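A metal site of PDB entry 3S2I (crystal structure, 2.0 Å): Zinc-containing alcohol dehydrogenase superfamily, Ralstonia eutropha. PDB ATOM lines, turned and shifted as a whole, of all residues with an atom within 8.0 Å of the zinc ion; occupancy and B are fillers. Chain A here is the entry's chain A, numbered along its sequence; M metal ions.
O of Cys 108 is in hydrogen-bond range of NE2 of Gln 111 (3.0 Å).
N of Gly 95 sits close to SG of Cys 100, at 3.1 Å.
SG of Cys 94 lies close to N of Tyr 96 (3.2 Å).
SG of Cys 97 sits close to N of His 99, 3.4 Å away.
The backbone NH (N) of Lys 110 lies close to the side-chain sulfur (SG) of Cys 108.
Merely in contact with the zinc ion: Gly 95 (3.7 Å).
Five residues have an atom within 4 Å of the zinc ion: Cys 94, Gly 95, Cys 97, Cys 100 and Cys 108.
The nearest printed residue that does not touch the zinc ion is Tyr 96 (4.4 Å).
The zinc ion is bound by the side-chain sulfur of Cys 94 (2.3 Å), the side-chain sulfur of Cys 100 (2.3 Å), the side-chain sulfur of Cys 108 (2.4 Å) and the side-chain sulfur of Cys 97 (2.5 Å).
The zinc ion has four donor atoms within binding distance.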
ATOM      1  N   SER A  92     -21.685   8.934 -30.401  1.00  0.00           N
ATOM      2  CA  SER A  92     -22.472   9.184 -29.203  1.00  0.00           C
ATOM      3  C   SER A  92     -23.311   7.945 -28.871  1.00  0.00           C
ATOM      4  O   SER A  92     -23.689   7.180 -29.751  1.00  0.00           O
ATOM      5  CB  SER A  92     -23.396  10.382 -29.410  1.00  0.00           C
ATOM      6  OG  SER A  92     -24.326  10.133 -30.451  1.00  0.00           O
ATOM      7  N   ALA A  93     -23.587   7.783 -27.584  1.00  0.00           N
ATOM      8  CA  ALA A  93     -24.538   6.776 -27.114  1.00  0.00           C
ATOM      9  C   ALA A  93     -25.580   7.489 -26.264  1.00  0.00           C
ATOM     10  O   ALA A  93     -25.407   8.656 -25.922  1.00  0.00           O
ATOM     11  CB  ALA A  93     -23.825   5.700 -26.320  1.00  0.00           C
ATOM     12  N   CYS A  94     -26.657   6.782 -25.933  1.00  0.00           N
ATOM     13  CA  CYS A  94     -27.768   7.413 -25.232  1.00  0.00           C
ATOM     14  C   CYS A  94     -27.433   7.742 -23.779  1.00  0.00           C
ATOM     15  O   CYS A  94     -27.909   8.732 -23.233  1.00  0.00           O
ATOM     16  CB  CYS A  94     -29.018   6.530 -25.301  1.00  0.00           C
ATOM     17  SG  CYS A  94     -29.000   5.207 -24.100  1.00  0.00           S
ATOM     18  N   GLY A  95     -26.630   6.893 -23.157  1.00  0.00           N
ATOM     19  CA  GLY A  95     -26.193   7.114 -21.790  1.00  0.00           C
ATOM     20  C   GLY A  95     -27.174   6.656 -20.724  1.00  0.00           C
ATOM     21  O   GLY A  95     -26.879   6.739 -19.528  1.00  0.00           O
ATOM     22  N   TYR A  96     -28.341   6.182 -21.142  1.00  0.00           N
ATOM     23  CA  TYR A  96     -29.412   5.826 -20.217  1.00  0.00           C
ATOM     24  C   TYR A  96     -29.677   4.326 -20.142  1.00  0.00           C
ATOM     25  O   TYR A  96     -30.117   3.817 -19.113  1.00  0.00           O
ATOM     26  CB  TYR A  96     -30.728   6.509 -20.629  1.00  0.00           C
ATOM     27  CG  TYR A  96     -30.619   7.988 -20.882  1.00  0.00           C
ATOM     28  CD1 TYR A  96     -29.698   8.774 -20.206  1.00  0.00           C
ATOM     29  CD2 TYR A  96     -31.452   8.602 -21.818  1.00  0.00           C
ATOM     30  CE1 TYR A  96     -29.608  10.140 -20.440  1.00  0.00           C
ATOM     31  CE2 TYR A  96     -31.365   9.967 -22.062  1.00  0.00           C
ATOM     32  CZ  TYR A  96     -30.439  10.726 -21.374  1.00  0.00           C
ATOM     33  OH  TYR A  96     -30.361  12.082 -21.624  1.00  0.00           O
ATOM     34  N   CYS A  97     -29.409   3.636 -21.246  1.00  0.00           N
ATOM     35  CA  CYS A  97     -29.843   2.248 -21.392  1.00  0.00           C
ATOM     36  C   CYS A  97     -29.035   1.252 -20.575  1.00  0.00           C
ATOM     37  O   CYS A  97     -28.011   1.590 -19.978  1.00  0.00           O
ATOM     38  CB  CYS A  97     -29.827   1.827 -22.877  1.00  0.00           C
ATOM     39  SG  CYS A  97     -28.185   1.479 -23.522  1.00  0.00           S
ATOM     40  N   GLU A  98     -29.512   0.003 -20.564  1.00  0.00           N
ATOM     41  CA  GLU A  98     -28.828  -1.092 -19.886  1.00  0.00           C
ATOM     42  C   GLU A  98     -27.350  -1.129 -20.267  1.00  0.00           C
ATOM     43  O   GLU A  98     -26.473  -1.176 -19.398  1.00  0.00           O
ATOM     44  CB  GLU A  98     -29.504  -2.422 -20.233  1.00  0.00           C
ATOM     45  CG  GLU A  98     -28.800  -3.646 -19.664  1.00  0.00           C
ATOM     46  CD  GLU A  98     -29.560  -4.939 -19.924  1.00  0.00           C
ATOM     47  OE1 GLU A  98     -29.934  -5.202 -21.085  1.00  0.00           O
ATOM     48  OE2 GLU A  98     -29.780  -5.702 -18.961  1.00  0.00           O
ATOM     49  N   HIS A  99     -27.085  -1.125 -21.564  1.00  0.00           N
ATOM     50  CA  HIS A  99     -25.715  -1.222 -22.051  1.00  0.00           C
ATOM     51  C   HIS A  99     -24.870  -0.015 -21.618  1.00  0.00           C
ATOM     52  O   HIS A  99     -23.752  -0.186 -21.134  1.00  0.00           O
ATOM     53  CB  HIS A  99     -25.701  -1.355 -23.577  1.00  0.00           C
ATOM     54  CG  HIS A  99     -26.479  -2.535 -24.077  1.00  0.00           C
ATOM     55  ND1 HIS A  99     -26.148  -3.828 -23.758  1.00  0.00           N
ATOM     56  CD2 HIS A  99     -27.566  -2.609 -24.873  1.00  0.00           C
ATOM     57  CE1 HIS A  99     -27.006  -4.659 -24.344  1.00  0.00           C
ATOM     58  NE2 HIS A  99     -27.877  -3.940 -25.025  1.00  0.00           N
ATOM     59  N   CYS A 100     -25.424   1.184 -21.790  1.00  0.00           N
ATOM     60  CA  CYS A 100     -24.715   2.417 -21.442  1.00  0.00           C
ATOM     61  C   CYS A 100     -24.355   2.529 -19.963  1.00  0.00           C
ATOM     62  O   CYS A 100     -23.331   3.102 -19.604  1.00  0.00           O
ATOM     63  CB  CYS A 100     -25.518   3.647 -21.863  1.00  0.00           C
ATOM     64  SG  CYS A 100     -25.353   4.053 -23.605  1.00  0.00           S
ATOM     65  N   LEU A 101     -25.217   1.982 -19.107  1.00  0.00           N
ATOM     66  CA  LEU A 101     -24.995   2.061 -17.664  1.00  0.00           C
ATOM     67  C   LEU A 101     -24.082   0.958 -17.167  1.00  0.00           C
ATOM     68  O   LEU A 101     -23.584   1.021 -16.036  1.00  0.00           O
ATOM     69  CB  LEU A 101     -26.324   2.034 -16.912  1.00  0.00           C
ATOM     70  CG  LEU A 101     -27.302   3.161 -17.242  1.00  0.00           C
ATOM     71  CD1 LEU A 101     -28.632   2.937 -16.541  1.00  0.00           C
ATOM     72  CD2 LEU A 101     -26.714   4.508 -16.866  1.00  0.00           C
ATOM     73  N   TRP A 104     -20.883  -0.550 -21.327  1.00  0.00           N
ATOM     74  CA  TRP A 104     -20.859  -1.149 -22.656  1.00  0.00           C
ATOM     75  C   TRP A 104     -21.554  -0.249 -23.680  1.00  0.00           C
ATOM     76  O   TRP A 104     -22.437  -0.702 -24.406  1.00  0.00           O
ATOM     77  CB  TRP A 104     -21.506  -2.538 -22.636  1.00  0.00           C
ATOM     78  CG  TRP A 104     -20.626  -3.607 -22.058  1.00  0.00           C
ATOM     79  CD1 TRP A 104     -20.661  -4.102 -20.783  1.00  0.00           C
ATOM     80  CD2 TRP A 104     -19.576  -4.325 -22.730  1.00  0.00           C
ATOM     81  NE1 TRP A 104     -19.702  -5.074 -20.623  1.00  0.00           N
ATOM     82  CE2 TRP A 104     -19.020  -5.230 -21.807  1.00  0.00           C
ATOM     83  CE3 TRP A 104     -19.060  -4.276 -24.030  1.00  0.00           C
ATOM     84  CZ2 TRP A 104     -17.976  -6.082 -22.134  1.00  0.00           C
ATOM     85  CZ3 TRP A 104     -18.016  -5.128 -24.357  1.00  0.00           C
ATOM     86  CH2 TRP A 104     -17.485  -6.019 -23.417  1.00  0.00           C
ATOM     87  N   GLU A 105     -21.165   1.019 -23.728  1.00  0.00           N
ATOM     88  CA  GLU A 105     -21.806   1.986 -24.608  1.00  0.00           C
ATOM     89  C   GLU A 105     -21.634   1.626 -26.087  1.00  0.00           C
ATOM     90  O   GLU A 105     -22.361   2.111 -26.948  1.00  0.00           O
ATOM     91  CB  GLU A 105     -21.295   3.397 -24.341  1.00  0.00           C
ATOM     92  CG  GLU A 105     -19.802   3.593 -24.584  1.00  0.00           C
ATOM     93  CD  GLU A 105     -19.047   3.817 -23.291  1.00  0.00           C
ATOM     94  OE1 GLU A 105     -19.378   3.149 -22.291  1.00  0.00           O
ATOM     95  OE2 GLU A 105     -18.122   4.674 -23.260  1.00  0.00           O
ATOM     96  N   THR A 106     -20.641   0.781 -26.366  1.00  0.00           N
ATOM     97  CA  THR A 106     -20.402   0.315 -27.729  1.00  0.00           C
ATOM     98  C   THR A 106     -21.583  -0.504 -28.252  1.00  0.00           C
ATOM     99  O   THR A 106     -21.737  -0.685 -29.463  1.00  0.00           O
ATOM    100  CB  THR A 106     -19.137  -0.542 -27.800  1.00  0.00           C
ATOM    101  OG1 THR A 106     -19.074  -1.367 -26.627  1.00  0.00           O
ATOM    102  CG2 THR A 106     -17.905   0.336 -27.851  1.00  0.00           C
ATOM    103  N   LEU A 107     -22.418  -0.965 -27.329  1.00  0.00           N
ATOM    104  CA  LEU A 107     -23.542  -1.822 -27.687  1.00  0.00           C
ATOM    105  C   LEU A 107     -24.869  -1.074 -27.679  1.00  0.00           C
ATOM    106  O   LEU A 107     -25.927  -1.653 -27.919  1.00  0.00           O
ATOM    107  CB  LEU A 107     -23.621  -3.024 -26.733  1.00  0.00           C
ATOM    108  CG  LEU A 107     -22.385  -3.920 -26.652  1.00  0.00           C
ATOM    109  CD1 LEU A 107     -22.605  -5.026 -25.619  1.00  0.00           C
ATOM    110  CD2 LEU A 107     -22.064  -4.508 -28.007  1.00  0.00           C
ATOM    111  N   CYS A 108     -24.811   0.226 -27.419  1.00  0.00           N
ATOM    112  CA  CYS A 108     -26.015   1.031 -27.351  1.00  0.00           C
ATOM    113  C   CYS A 108     -26.803   0.982 -28.652  1.00  0.00           C
ATOM    114  O   CYS A 108     -26.288   1.287 -29.726  1.00  0.00           O
ATOM    115  CB  CYS A 108     -25.675   2.479 -27.011  1.00  0.00           C
ATOM    116  SG  CYS A 108     -27.126   3.541 -26.890  1.00  0.00           S
ATOM    117  N   GLU A 109     -28.081   0.604 -28.546  1.00  0.00           N
ATOM    118  CA  GLU A 109     -28.959   0.483 -29.703  1.00  0.00           C
ATOM    119  C   GLU A 109     -29.166   1.833 -30.377  1.00  0.00           C
ATOM    120  O   GLU A 109     -29.471   1.899 -31.565  1.00  0.00           O
ATOM    121  CB  GLU A 109     -30.311  -0.080 -29.286  1.00  0.00           C
ATOM    122  CG  GLU A 109     -30.229  -1.393 -28.510  1.00  0.00           C
ATOM    123  CD  GLU A 109     -30.367  -2.612 -29.399  1.00  0.00           C
ATOM    124  OE1 GLU A 109     -30.395  -3.734 -28.862  1.00  0.00           O
ATOM    125  OE2 GLU A 109     -30.446  -2.442 -30.632  1.00  0.00           O
ATOM    126  N   LYS A 110     -28.979   2.910 -29.605  1.00  0.00           N
ATOM    127  CA  LYS A 110     -29.222   4.265 -30.099  1.00  0.00           C
ATOM    128  C   LYS A 110     -27.959   5.009 -30.496  1.00  0.00           C
ATOM    129  O   LYS A 110     -27.990   6.207 -30.756  1.00  0.00           O
ATOM    130  CB  LYS A 110     -29.957   5.090 -29.035  1.00  0.00           C
ATOM    131  CG  LYS A 110     -31.422   4.742 -28.838  1.00  0.00           C
ATOM    132  CD  LYS A 110     -32.079   5.720 -27.880  1.00  0.00           C
ATOM    133  CE  LYS A 110     -33.547   5.408 -27.665  1.00  0.00           C
ATOM    134  NZ  LYS A 110     -34.341   5.578 -28.914  1.00  0.00           N
ATOM    135  N   GLN A 111     -26.835   4.293 -30.546  1.00  0.00           N
ATOM    136  CA  GLN A 111     -25.560   4.939 -30.851  1.00  0.00           C
ATOM    137  C   GLN A 111     -25.569   5.577 -32.244  1.00  0.00           C
ATOM    138  O   GLN A 111     -26.341   5.176 -33.119  1.00  0.00           O
ATOM    139  CB  GLN A 111     -24.405   3.948 -30.733  1.00  0.00           C
ATOM    140  CG  GLN A 111     -24.366   2.913 -31.850  1.00  0.00           C
ATOM    141  CD  GLN A 111     -23.261   1.897 -31.659  1.00  0.00           C
ATOM    142  OE1 GLN A 111     -22.162   2.055 -32.190  1.00  0.00           O
ATOM    143  NE2 GLN A 111     -23.541   0.850 -30.888  1.00  0.00           N
ATOM    144  N   TYR A 132     -17.777  12.092 -25.916  1.00  0.00           N
ATOM    145  CA  TYR A 132     -17.416  10.849 -26.586  1.00  0.00           C
ATOM    146  C   TYR A 132     -16.121  10.897 -27.393  1.00  0.00           C
ATOM    147  O   TYR A 132     -15.591   9.859 -27.804  1.00  0.00           O
ATOM    148  CB  TYR A 132     -18.578  10.356 -27.459  1.00  0.00           C
ATOM    149  CG  TYR A 132     -19.731   9.859 -26.618  1.00  0.00           C
ATOM    150  CD1 TYR A 132     -20.730  10.722 -26.201  1.00  0.00           C
ATOM    151  CD2 TYR A 132     -19.790   8.545 -26.219  1.00  0.00           C
ATOM    152  CE1 TYR A 132     -21.779  10.277 -25.422  1.00  0.00           C
ATOM    153  CE2 TYR A 132     -20.831   8.078 -25.440  1.00  0.00           C
ATOM    154  CZ  TYR A 132     -21.821   8.955 -25.038  1.00  0.00           C
ATOM    155  OH  TYR A 132     -22.862   8.503 -24.260  1.00  0.00           O
HETATM  156 ZN    ZN M   1     -27.451   3.618 -24.544  1.00  0.00          ZN
